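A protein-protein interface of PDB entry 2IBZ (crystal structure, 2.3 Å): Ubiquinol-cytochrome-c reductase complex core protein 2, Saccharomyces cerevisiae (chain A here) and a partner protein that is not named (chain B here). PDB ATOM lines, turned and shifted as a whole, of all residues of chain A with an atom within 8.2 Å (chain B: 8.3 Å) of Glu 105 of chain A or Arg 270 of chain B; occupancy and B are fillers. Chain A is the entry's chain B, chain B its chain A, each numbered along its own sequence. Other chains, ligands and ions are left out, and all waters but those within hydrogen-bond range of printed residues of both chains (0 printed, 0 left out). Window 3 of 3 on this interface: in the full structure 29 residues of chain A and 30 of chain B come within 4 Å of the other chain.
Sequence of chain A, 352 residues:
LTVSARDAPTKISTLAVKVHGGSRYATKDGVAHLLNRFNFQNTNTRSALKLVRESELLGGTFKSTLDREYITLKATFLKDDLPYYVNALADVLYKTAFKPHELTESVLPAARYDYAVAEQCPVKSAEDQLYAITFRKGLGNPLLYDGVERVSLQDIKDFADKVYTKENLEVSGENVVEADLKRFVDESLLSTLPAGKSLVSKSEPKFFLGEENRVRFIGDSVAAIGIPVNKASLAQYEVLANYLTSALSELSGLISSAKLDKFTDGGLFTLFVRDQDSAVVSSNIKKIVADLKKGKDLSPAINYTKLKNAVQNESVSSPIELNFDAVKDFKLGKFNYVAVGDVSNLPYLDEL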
ATOM      1  N   GLN A  41       6.267  22.533 -22.812  1.00  0.00           N
ATOM      2  CA  GLN A  41       6.472  23.656 -21.914  1.00  0.00           C
ATOM      3  C   GLN A  41       5.053  24.023 -21.478  1.00  0.00           C
ATOM      4  O   GLN A  41       4.164  23.161 -21.445  1.00  0.00           O
ATOM      5  CB  GLN A  41       7.125  24.832 -22.639  1.00  0.00           C
ATOM      6  CG  GLN A  41       8.639  24.709 -22.797  1.00  0.00           C
ATOM      7  CD  GLN A  41       9.390  24.640 -21.462  1.00  0.00           C
ATOM      8  OE1 GLN A  41      10.335  23.871 -21.314  1.00  0.00           O
ATOM      9  NE2 GLN A  41       8.976  25.452 -20.498  1.00  0.00           N
ATOM     10  N   LEU A  49       4.817  22.018 -15.407  1.00  0.00           N
ATOM     11  CA  LEU A  49       4.890  21.348 -14.114  1.00  0.00           C
ATOM     12  C   LEU A  49       3.702  20.402 -13.877  1.00  0.00           C
ATOM     13  O   LEU A  49       3.887  19.220 -13.564  1.00  0.00           O
ATOM     14  CB  LEU A  49       4.981  22.392 -12.988  1.00  0.00           C
ATOM     15  CG  LEU A  49       4.801  21.922 -11.545  1.00  0.00           C
ATOM     16  CD1 LEU A  49       5.946  21.025 -11.119  1.00  0.00           C
ATOM     17  CD2 LEU A  49       4.712  23.135 -10.643  1.00  0.00           C
ATOM     18  N   VAL A  52       3.579  17.135 -16.063  1.00  0.00           N
ATOM     19  CA  VAL A  52       4.476  16.121 -15.526  1.00  0.00           C
ATOM     20  C   VAL A  52       3.900  15.506 -14.252  1.00  0.00           C
ATOM     21  O   VAL A  52       3.818  14.288 -14.109  1.00  0.00           O
ATOM     22  CB  VAL A  52       5.874  16.720 -15.220  1.00  0.00           C
ATOM     23  CG1 VAL A  52       6.758  15.703 -14.518  1.00  0.00           C
ATOM     24  CG2 VAL A  52       6.534  17.206 -16.496  1.00  0.00           C
ATOM     25  N   ARG A  53       3.463  16.341 -13.328  1.00  0.00           N
ATOM     26  CA  ARG A  53       2.931  15.807 -12.087  1.00  0.00           C
ATOM     27  C   ARG A  53       1.722  14.919 -12.331  1.00  0.00           C
ATOM     28  O   ARG A  53       1.605  13.865 -11.713  1.00  0.00           O
ATOM     29  CB  ARG A  53       2.620  16.934 -11.101  1.00  0.00           C
ATOM     30  CG  ARG A  53       3.772  17.923 -10.979  1.00  0.00           C
ATOM     31  CD  ARG A  53       5.044  17.245 -10.488  1.00  0.00           C
ATOM     32  NE  ARG A  53       4.987  17.112  -9.046  1.00  0.00           N
ATOM     33  CZ  ARG A  53       5.690  17.853  -8.196  1.00  0.00           C
ATOM     34  NH1 ARG A  53       5.524  17.671  -6.897  1.00  0.00           N
ATOM     35  NH2 ARG A  53       6.607  18.704  -8.634  1.00  0.00           N
ATOM     36  N   GLU A  56       2.693  11.562 -14.250  1.00  0.00           N
ATOM     37  CA  GLU A  56       3.422  10.659 -13.361  1.00  0.00           C
ATOM     38  C   GLU A  56       2.462   9.823 -12.528  1.00  0.00           C
ATOM     39  O   GLU A  56       2.686   8.631 -12.333  1.00  0.00           O
ATOM     40  CB  GLU A  56       4.359  11.431 -12.418  1.00  0.00           C
ATOM     41  CG  GLU A  56       5.544  12.110 -13.100  1.00  0.00           C
ATOM     42  CD  GLU A  56       6.577  12.690 -12.121  1.00  0.00           C
ATOM     43  OE1 GLU A  56       6.286  12.864 -10.916  1.00  0.00           O
ATOM     44  OE2 GLU A  56       7.702  12.958 -12.576  1.00  0.00           O
ATOM     45  N   LYS A  99       5.891  31.794 -23.640  1.00  0.00           N
ATOM     46  CA  LYS A  99       6.242  32.945 -22.804  1.00  0.00           C
ATOM     47  C   LYS A  99       7.721  33.292 -22.994  1.00  0.00           C
ATOM     48  O   LYS A  99       8.559  32.402 -23.075  1.00  0.00           O
ATOM     49  CB  LYS A  99       5.969  32.628 -21.329  1.00  0.00           C
ATOM     50  CG  LYS A  99       4.517  32.260 -21.023  1.00  0.00           C
ATOM     51  CD  LYS A  99       3.575  33.409 -21.349  1.00  0.00           C
ATOM     52  CE  LYS A  99       3.098  34.125 -20.095  1.00  0.00           C
ATOM     53  NZ  LYS A  99       2.166  33.272 -19.294  1.00  0.00           N
ATOM     54  N   PRO A 100       8.063  34.591 -23.050  1.00  0.00           N
ATOM     55  CA  PRO A 100       9.456  35.027 -23.232  1.00  0.00           C
ATOM     56  C   PRO A 100      10.423  34.469 -22.181  1.00  0.00           C
ATOM     57  O   PRO A 100      11.595  34.233 -22.472  1.00  0.00           O
ATOM     58  CB  PRO A 100       9.363  36.556 -23.118  1.00  0.00           C
ATOM     59  CG  PRO A 100       7.969  36.854 -23.548  1.00  0.00           C
ATOM     60  CD  PRO A 100       7.170  35.751 -22.889  1.00  0.00           C
ATOM     61  N   HIS A 101       9.932  34.257 -20.961  1.00  0.00           N
ATOM     62  CA  HIS A 101      10.785  33.745 -19.902  1.00  0.00           C
ATOM     63  C   HIS A 101      11.029  32.251 -20.030  1.00  0.00           C
ATOM     64  O   HIS A 101      12.003  31.734 -19.483  1.00  0.00           O
ATOM     65  CB  HIS A 101      10.230  34.097 -18.520  1.00  0.00           C
ATOM     66  CG  HIS A 101       9.010  33.324 -18.124  1.00  0.00           C
ATOM     67  ND1 HIS A 101       7.751  33.883 -18.101  1.00  0.00           N
ATOM     68  CD2 HIS A 101       8.867  32.057 -17.664  1.00  0.00           C
ATOM     69  CE1 HIS A 101       6.887  32.998 -17.637  1.00  0.00           C
ATOM     70  NE2 HIS A 101       7.538  31.881 -17.365  1.00  0.00           N
ATOM     71  N   GLU A 102      10.122  31.549 -20.710  1.00  0.00           N
ATOM     72  CA  GLU A 102      10.289  30.110 -20.919  1.00  0.00           C
ATOM     73  C   GLU A 102      11.407  29.930 -21.925  1.00  0.00           C
ATOM     74  O   GLU A 102      12.159  28.963 -21.871  1.00  0.00           O
ATOM     75  CB  GLU A 102       9.013  29.477 -21.445  1.00  0.00           C
ATOM     76  CG  GLU A 102       7.872  29.557 -20.472  1.00  0.00           C
ATOM     77  CD  GLU A 102       6.720  28.682 -20.879  1.00  0.00           C
ATOM     78  OE1 GLU A 102       5.920  29.118 -21.735  1.00  0.00           O
ATOM     79  OE2 GLU A 102       6.625  27.557 -20.347  1.00  0.00           O
ATOM     80  N   LEU A 103      11.529  30.899 -22.822  1.00  0.00           N
ATOM     81  CA  LEU A 103      12.565  30.863 -23.830  1.00  0.00           C
ATOM     82  C   LEU A 103      13.926  30.927 -23.143  1.00  0.00           C
ATOM     83  O   LEU A 103      14.708  29.973 -23.206  1.00  0.00           O
ATOM     84  CB  LEU A 103      12.404  32.033 -24.810  1.00  0.00           C
ATOM     85  CG  LEU A 103      13.468  32.130 -25.908  1.00  0.00           C
ATOM     86  CD1 LEU A 103      13.553  30.810 -26.664  1.00  0.00           C
ATOM     87  CD2 LEU A 103      13.165  33.291 -26.853  1.00  0.00           C
ATOM     88  N   THR A 104      14.156  32.029 -22.427  1.00  0.00           N
ATOM     89  CA  THR A 104      15.420  32.280 -21.727  1.00  0.00           C
ATOM     90  C   THR A 104      15.803  31.327 -20.589  1.00  0.00           C
ATOM     91  O   THR A 104      16.978  31.014 -20.414  1.00  0.00           O
ATOM     92  CB  THR A 104      15.465  33.719 -21.181  1.00  0.00           C
ATOM     93  OG1 THR A 104      14.360  33.919 -20.299  1.00  0.00           O
ATOM     94  CG2 THR A 104      15.379  34.733 -22.307  1.00  0.00           C
ATOM     95  N   GLU A 105      14.816  30.834 -19.854  1.00  0.00           N
ATOM     96  CA  GLU A 105      15.072  29.954 -18.722  1.00  0.00           C
ATOM     97  C   GLU A 105      15.099  28.454 -18.964  1.00  0.00           C
ATOM     98  O   GLU A 105      15.752  27.737 -18.208  1.00  0.00           O
ATOM     99  CB  GLU A 105      14.076  30.240 -17.593  1.00  0.00           C
ATOM    100  CG  GLU A 105      14.113  31.662 -17.077  1.00  0.00           C
ATOM    101  CD  GLU A 105      13.040  31.946 -16.041  1.00  0.00           C
ATOM    102  OE1 GLU A 105      12.346  30.996 -15.594  1.00  0.00           O
ATOM    103  OE2 GLU A 105      12.889  33.132 -15.678  1.00  0.00           O
ATOM    104  N   SER A 106      14.381  27.967 -19.976  1.00  0.00           N
ATOM    105  CA  SER A 106      14.338  26.524 -20.234  1.00  0.00           C
ATOM    106  C   SER A 106      14.696  26.064 -21.634  1.00  0.00           C
ATOM    107  O   SER A 106      15.380  25.054 -21.791  1.00  0.00           O
ATOM    108  CB  SER A 106      12.965  25.953 -19.886  1.00  0.00           C
ATOM    109  OG  SER A 106      12.606  26.261 -18.553  1.00  0.00           O
ATOM    110  N   VAL A 107      14.211  26.783 -22.644  1.00  0.00           N
ATOM    111  CA  VAL A 107      14.447  26.423 -24.041  1.00  0.00           C
ATOM    112  C   VAL A 107      15.874  26.660 -24.522  1.00  0.00           C
ATOM    113  O   VAL A 107      16.515  25.738 -25.038  1.00  0.00           O
ATOM    114  CB  VAL A 107      13.424  27.126 -24.976  1.00  0.00           C
ATOM    115  CG1 VAL A 107      13.728  26.825 -26.445  1.00  0.00           C
ATOM    116  CG2 VAL A 107      12.020  26.659 -24.631  1.00  0.00           C
ATOM    117  N   LEU A 108      16.364  27.885 -24.371  1.00  0.00           N
ATOM    118  CA  LEU A 108      17.725  28.202 -24.782  1.00  0.00           C
ATOM    119  C   LEU A 108      18.770  27.334 -24.060  1.00  0.00           C
ATOM    120  O   LEU A 108      19.692  26.834 -24.690  1.00  0.00           O
ATOM    121  CB  LEU A 108      18.020  29.695 -24.600  1.00  0.00           C
ATOM    122  CG  LEU A 108      17.286  30.609 -25.583  1.00  0.00           C
ATOM    123  CD1 LEU A 108      17.677  32.078 -25.370  1.00  0.00           C
ATOM    124  CD2 LEU A 108      17.617  30.172 -27.012  1.00  0.00           C
ATOM    125  N   PRO A 109      18.658  27.172 -22.724  1.00  0.00           N
ATOM    126  CA  PRO A 109      19.642  26.339 -22.018  1.00  0.00           C
ATOM    127  C   PRO A 109      19.624  24.897 -22.516  1.00  0.00           C
ATOM    128  O   PRO A 109      20.676  24.319 -22.784  1.00  0.00           O
ATOM    129  CB  PRO A 109      19.180  26.427 -20.561  1.00  0.00           C
ATOM    130  CG  PRO A 109      18.676  27.822 -20.488  1.00  0.00           C
ATOM    131  CD  PRO A 109      17.849  27.932 -21.751  1.00  0.00           C
ATOM    132  N   ALA A 110      18.428  24.331 -22.661  1.00  0.00           N
ATOM    133  CA  ALA A 110      18.287  22.949 -23.125  1.00  0.00           C
ATOM    134  C   ALA A 110      18.864  22.768 -24.521  1.00  0.00           C
ATOM    135  O   ALA A 110      19.482  21.750 -24.809  1.00  0.00           O
ATOM    136  CB  ALA A 110      16.834  22.519 -23.092  1.00  0.00           C
ATOM    137  N   SER B 261      15.316   8.708 -11.130  1.00  0.00           N
ATOM    138  CA  SER B 261      16.528   9.174 -11.766  1.00  0.00           C
ATOM    139  C   SER B 261      16.369  10.626 -12.155  1.00  0.00           C
ATOM    140  O   SER B 261      15.253  11.135 -12.214  1.00  0.00           O
ATOM    141  CB  SER B 261      16.912   8.271 -12.955  1.00  0.00           C
ATOM    142  OG  SER B 261      16.089   8.493 -14.080  1.00  0.00           O
ATOM    143  N   TYR B 262      17.483  11.299 -12.407  1.00  0.00           N
ATOM    144  CA  TYR B 262      17.445  12.713 -12.722  1.00  0.00           C
ATOM    145  C   TYR B 262      18.523  13.147 -13.702  1.00  0.00           C
ATOM    146  O   TYR B 262      19.583  12.549 -13.770  1.00  0.00           O
ATOM    147  CB  TYR B 262      17.542  13.491 -11.401  1.00  0.00           C
ATOM    148  CG  TYR B 262      17.851  14.965 -11.513  1.00  0.00           C
ATOM    149  CD1 TYR B 262      19.149  15.439 -11.310  1.00  0.00           C
ATOM    150  CD2 TYR B 262      16.847  15.892 -11.773  1.00  0.00           C
ATOM    151  CE1 TYR B 262      19.436  16.801 -11.363  1.00  0.00           C
ATOM    152  CE2 TYR B 262      17.126  17.259 -11.825  1.00  0.00           C
ATOM    153  CZ  TYR B 262      18.425  17.702 -11.619  1.00  0.00           C
ATOM    154  OH  TYR B 262      18.711  19.047 -11.686  1.00  0.00           O
ATOM    155  N   ASN B 263      18.238  14.207 -14.442  1.00  0.00           N
ATOM    156  CA  ASN B 263      19.154  14.754 -15.430  1.00  0.00           C
ATOM    157  C   ASN B 263      18.898  16.262 -15.414  1.00  0.00           C
ATOM    158  O   ASN B 263      17.886  16.738 -15.929  1.00  0.00           O
ATOM    159  CB  ASN B 263      18.841  14.161 -16.811  1.00  0.00           C
ATOM    160  CG  ASN B 263      19.806  14.631 -17.908  1.00  0.00           C
ATOM    161  OD1 ASN B 263      19.972  13.940 -18.918  1.00  0.00           O
ATOM    162  ND2 ASN B 263      20.428  15.803 -17.728  1.00  0.00           N
ATOM    163  N   ALA B 264      19.833  16.998 -14.825  1.00  0.00           N
ATOM    164  CA  ALA B 264      19.748  18.445 -14.688  1.00  0.00           C
ATOM    165  C   ALA B 264      19.588  19.244 -15.970  1.00  0.00           C
ATOM    166  O   ALA B 264      19.176  20.399 -15.926  1.00  0.00           O
ATOM    167  CB  ALA B 264      20.957  18.953 -13.920  1.00  0.00           C
ATOM    168  N   PHE B 265      19.925  18.665 -17.113  1.00  0.00           N
ATOM    169  CA  PHE B 265      19.803  19.422 -18.361  1.00  0.00           C
ATOM    170  C   PHE B 265      18.460  19.270 -19.091  1.00  0.00           C
ATOM    171  O   PHE B 265      18.117  20.089 -19.953  1.00  0.00           O
ATOM    172  CB  PHE B 265      20.998  19.125 -19.265  1.00  0.00           C
ATOM    173  CG  PHE B 265      22.320  19.434 -18.612  1.00  0.00           C
ATOM    174  CD1 PHE B 265      23.006  18.452 -17.907  1.00  0.00           C
ATOM    175  CD2 PHE B 265      22.839  20.723 -18.639  1.00  0.00           C
ATOM    176  CE1 PHE B 265      24.193  18.754 -17.228  1.00  0.00           C
ATOM    177  CE2 PHE B 265      24.024  21.034 -17.963  1.00  0.00           C
ATOM    178  CZ  PHE B 265      24.701  20.046 -17.255  1.00  0.00           C
ATOM    179  N   GLU B 266      17.699  18.249 -18.692  1.00  0.00           N
ATOM    180  CA  GLU B 266      16.384  17.961 -19.257  1.00  0.00           C
ATOM    181  C   GLU B 266      15.293  18.674 -18.455  1.00  0.00           C
ATOM    182  O   GLU B 266      14.952  18.260 -17.343  1.00  0.00           O
ATOM    183  CB  GLU B 266      16.117  16.442 -19.270  1.00  0.00           C
ATOM    184  CG  GLU B 266      16.809  15.675 -20.394  1.00  0.00           C
ATOM    185  CD  GLU B 266      16.384  16.142 -21.787  1.00  0.00           C
ATOM    186  OE1 GLU B 266      17.255  16.246 -22.679  1.00  0.00           O
ATOM    187  OE2 GLU B 266      15.178  16.412 -21.991  1.00  0.00           O
ATOM    188  N   PRO B 267      14.714  19.743 -19.027  1.00  0.00           N
ATOM    189  CA  PRO B 267      13.654  20.553 -18.412  1.00  0.00           C
ATOM    190  C   PRO B 267      12.594  19.734 -17.672  1.00  0.00           C
ATOM    191  O   PRO B 267      12.270  20.002 -16.510  1.00  0.00           O
ATOM    192  CB  PRO B 267      13.061  21.277 -19.611  1.00  0.00           C
ATOM    193  CG  PRO B 267      14.289  21.549 -20.454  1.00  0.00           C
ATOM    194  CD  PRO B 267      15.012  20.219 -20.393  1.00  0.00           C
ATOM    195  N   ALA B 268      12.098  18.699 -18.335  1.00  0.00           N
ATOM    196  CA  ALA B 268      11.073  17.841 -17.751  1.00  0.00           C
ATOM    197  C   ALA B 268      11.547  17.101 -16.519  1.00  0.00           C
ATOM    198  O   ALA B 268      10.752  16.817 -15.625  1.00  0.00           O
ATOM    199  CB  ALA B 268      10.571  16.838 -18.786  1.00  0.00           C
ATOM    200  N   SER B 269      12.826  16.744 -16.489  1.00  0.00           N
ATOM    201  CA  SER B 269      13.375  15.995 -15.353  1.00  0.00           C
ATOM    202  C   SER B 269      13.385  16.822 -14.073  1.00  0.00           C
ATOM    203  O   SER B 269      13.158  16.298 -12.979  1.00  0.00           O
ATOM    204  CB  SER B 269      14.785  15.490 -15.673  1.00  0.00           C
ATOM    205  OG  SER B 269      15.176  14.460 -14.777  1.00  0.00           O
ATOM    206  N   ARG B 270      13.599  18.124 -14.231  1.00  0.00           N
ATOM    207  CA  ARG B 270      13.638  19.058 -13.109  1.00  0.00           C
ATOM    208  C   ARG B 270      12.253  19.267 -12.492  1.00  0.00           C
ATOM    209  O   ARG B 270      12.132  19.873 -11.424  1.00  0.00           O
ATOM    210  CB  ARG B 270      14.194  20.410 -13.578  1.00  0.00           C
ATOM    211  CG  ARG B 270      15.438  20.298 -14.458  1.00  0.00           C
ATOM    212  CD  ARG B 270      16.307  21.540 -14.396  1.00  0.00           C
ATOM    213  NE  ARG B 270      15.760  22.647 -15.166  1.00  0.00           N
ATOM    214  CZ  ARG B 270      16.421  23.292 -16.132  1.00  0.00           C
ATOM    215  NH1 ARG B 270      15.839  24.298 -16.789  1.00  0.00           N
ATOM    216  NH2 ARG B 270      17.665  22.934 -16.450  1.00  0.00           N
ATOM    217  N   LEU B 271      11.213  18.747 -13.149  1.00  0.00           N
ATOM    218  CA  LEU B 271       9.846  18.932 -12.666  1.00  0.00           C
ATOM    219  C   LEU B 271       9.207  17.728 -11.976  1.00  0.00           C
ATOM    220  O   LEU B 271       8.103  17.828 -11.452  1.00  0.00           O
ATOM    221  CB  LEU B 271       8.960  19.415 -13.812  1.00  0.00           C
ATOM    222  CG  LEU B 271       9.460  20.641 -14.587  1.00  0.00           C
ATOM    223  CD1 LEU B 271       8.653  20.833 -15.890  1.00  0.00           C
ATOM    224  CD2 LEU B 271       9.385  21.885 -13.705  1.00  0.00           C
ATOM    225  N   GLN B 272       9.905  16.604 -11.937  1.00  0.00           N
ATOM    226  CA  GLN B 272       9.353  15.412 -11.302  1.00  0.00           C
ATOM    227  C   GLN B 272       8.920  15.577  -9.849  1.00  0.00           C
ATOM    228  O   GLN B 272       9.493  16.382  -9.091  1.00  0.00           O
ATOM    229  CB  GLN B 272      10.344  14.261 -11.382  1.00  0.00           C
ATOM    230  CG  GLN B 272      10.803  13.929 -12.777  1.00  0.00           C
ATOM    231  CD  GLN B 272      11.886  12.891 -12.754  1.00  0.00           C
ATOM    232  OE1 GLN B 272      11.648  11.740 -12.366  1.00  0.00           O
ATOM    233  NE2 GLN B 272      13.104  13.299 -13.106  1.00  0.00           N
ATOM    234  N   GLY B 273       7.966  14.736  -9.452  1.00  0.00           N
ATOM    235  CA  GLY B 273       7.432  14.745  -8.100  1.00  0.00           C
ATOM    236  C   GLY B 273       8.354  14.029  -7.137  1.00  0.00           C
ATOM    237  O   GLY B 273       7.986  13.009  -6.525  1.00  0.00           O
ATOM    238  N   ILE B 274       9.565  14.570  -7.004  1.00  0.00           N
ATOM    239  CA  ILE B 274      10.573  14.005  -6.115  1.00  0.00           C
ATOM    240  C   ILE B 274      11.044  15.105  -5.169  1.00  0.00           C
ATOM    241  O   ILE B 274      11.606  16.106  -5.607  1.00  0.00           O
ATOM    242  CB  ILE B 274      11.770  13.425  -6.929  1.00  0.00           C
ATOM    243  CG1 ILE B 274      11.264  12.343  -7.895  1.00  0.00           C
ATOM    244  CG2 ILE B 274      12.823  12.811  -5.989  1.00  0.00           C
ATOM    245  CD1 ILE B 274      12.276  11.897  -8.918  1.00  0.00           C
ATOM    246  N   LEU B 277      14.577  16.786  -5.109  1.00  0.00           N
ATOM    247  CA  LEU B 277      14.907  17.797  -6.117  1.00  0.00           C
ATOM    248  C   LEU B 277      14.860  19.237  -5.641  1.00  0.00           C
ATOM    249  O   LEU B 277      15.471  20.116  -6.259  1.00  0.00           O
ATOM    250  CB  LEU B 277      14.034  17.643  -7.357  1.00  0.00           C
ATOM    251  CG  LEU B 277      14.234  16.370  -8.168  1.00  0.00           C
ATOM    252  CD1 LEU B 277      13.462  16.524  -9.470  1.00  0.00           C
ATOM    253  CD2 LEU B 277      15.718  16.137  -8.457  1.00  0.00           C
ATOM    254  N   ASP B 278      14.093  19.490  -4.584  1.00  0.00           N
ATOM    255  CA  ASP B 278      14.011  20.838  -4.024  1.00  0.00           C
ATOM    256  C   ASP B 278      15.378  21.196  -3.418  1.00  0.00           C
ATOM    257  O   ASP B 278      15.870  22.315  -3.582  1.00  0.00           O
ATOM    258  CB  ASP B 278      12.918  20.918  -2.943  1.00  0.00           C
ATOM    259  CG  ASP B 278      11.507  20.768  -3.508  1.00  0.00           C
ATOM    260  OD1 ASP B 278      10.623  20.243  -2.785  1.00  0.00           O
ATOM    261  OD2 ASP B 278      11.279  21.172  -4.666  1.00  0.00           O
ATOM    262  N   ILE B 280      18.500  19.563  -4.103  1.00  0.00           N
ATOM    263  CA  ILE B 280      19.626  19.526  -5.008  1.00  0.00           C
ATOM    264  C   ILE B 280      19.692  20.548  -6.129  1.00  0.00           C
ATOM    265  O   ILE B 280      20.773  20.806  -6.650  1.00  0.00           O
ATOM    266  CB  ILE B 280      19.909  18.071  -5.524  1.00  0.00           C
ATOM    267  CG1 ILE B 280      19.068  17.717  -6.740  1.00  0.00           C
ATOM    268  CG2 ILE B 280      19.720  17.062  -4.419  1.00  0.00           C
ATOM    269  CD1 ILE B 280      19.743  18.130  -8.032  1.00  0.00           C
ATOM    270  N   GLN B 281      18.572  21.179  -6.468  1.00  0.00           N
ATOM    271  CA  GLN B 281      18.585  22.151  -7.556  1.00  0.00           C
ATOM    272  C   GLN B 281      19.003  23.561  -7.182  1.00  0.00           C
ATOM    273  O   GLN B 281      19.462  24.311  -8.043  1.00  0.00           O
ATOM    274  CB  GLN B 281      17.241  22.178  -8.273  1.00  0.00           C
ATOM    275  CG  GLN B 281      16.832  20.813  -8.788  1.00  0.00           C
ATOM    276  CD  GLN B 281      15.819  20.888  -9.903  1.00  0.00           C
ATOM    277  OE1 GLN B 281      16.180  20.803 -11.078  1.00  0.00           O
ATOM    278  NE2 GLN B 281      14.550  21.059  -9.550  1.00  0.00           N
ATOM    279  N   GLN B 284      22.644  23.291  -7.463  1.00  0.00           N
ATOM    280  CA  GLN B 284      22.964  22.320  -8.501  1.00  0.00           C
ATOM    281  C   GLN B 284      24.055  21.355  -8.064  1.00  0.00           C
ATOM    282  O   GLN B 284      25.170  21.352  -8.581  1.00  0.00           O
ATOM    283  CB  GLN B 284      23.328  23.001  -9.822  1.00  0.00           C
ATOM    284  CG  GLN B 284      23.071  22.079 -11.035  1.00  0.00           C
ATOM    285  CD  GLN B 284      21.659  21.470 -11.023  1.00  0.00           C
ATOM    286  OE1 GLN B 284      20.683  22.124 -11.406  1.00  0.00           O
ATOM    287  NE2 GLN B 284      21.549  20.225 -10.559  1.00  0.00           N
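Of the 19 printed residues of chain B, 5 touch a printed residue of chain A. Printed residues of chain B that touch a printed residue of chain A: Pro 267, Arg 270, Leu 271, Gln 272 and Gly 273. Hydrophobic or aromatic side chains of chain B that line the printed part of chain A: Pro 267. Among the printed residues, no Asp or Glu carboxylate lies within 4 Å of a Lys or Arg side-chain nitrogen of the other chain.
Of chain B, only Arg 270 comes within 4 Å of Glu 105 of chain A. Printed residues of chain A within 4 Å of Leu 271 of chain B: Leu 49, Val 52 and Arg 53. Of the printed residues of chain B, Arg 53 of chain A touches Leu 271 (3.3 Å), Gln 272 (3.7 Å) and Gly 273 (3.5 Å). Printed residues of chain A within 4 Å of Pro 267 of chain B: Ser 106 and Ala 110. Of the printed residues of chain B, Leu 49 of chain A touches Leu 271. Of the printed residues of chain A, Gln 272 of chain B touches Arg 53 (3.7 Å) and Glu 56 (3.2 Å). Pro 109 of chain A touches none of the printed residues of chain B. The nearest residue of chain B that does not touch Glu 105 of chain A is Pro 267 of chain B (6.7 Å). The nearest residue of chain A that does not touch Arg 270 of chain B is Ser 106 of chain A (4.2 Å). The nearest printed residue of chain A that does not touch Pro 267 of chain B is Gln 41 of chain A (4.1 Å).
Among the printed residues, pairs that only touch across the chains: Leu 49 of chain A with Leu 271 of chain B (3.9 Å), Val 52 of chain A with Leu 271 of chain B (3.97 Å), Arg 53 of chain A with Gln 272 of chain B (3.7 Å), Arg 53 of chain A with Gly 273 of chain B (3.5 Å), Glu 56 of chain A with Gln 272 of chain B (3.2 Å), Glu 105 of chain A with Arg 270 of chain B (3.7 Å), Ser 106 of chain A with Pro 267 of chain B (3.9 Å) and Ala 110 of chain A with Pro 267 of chain B (3.8 Å).
The side-chain hydroxyl of Ser 269 of chain B lies within hydrogen-bond range of the side-chain amide nitrogen of Gln 272 of chain B (2.9 Å). NE2 of Gln 281 of chain B is in hydrogen-bond range of O of Arg 270 of chain B (3.3 Å). The backbone carbonyl oxygen of Ser 261 of chain B sits at hydrogen-bond distance from the side-chain amide nitrogen of Gln 272 of chain B. O of Ala 264 of chain B is in hydrogen-bond range of NH2 of Arg 270 of chain B (3.0 Å).
The guanidinium group (NH2) of Arg 53 of chain A sits close to the backbone carbonyl oxygen (O) of Leu 271 of chain B (3.3 Å). The backbone NH of Gly 273 of chain B lies within hydrogen-bond range of the side-chain carboxylate of Glu 56 of chain A (2.9 Å).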
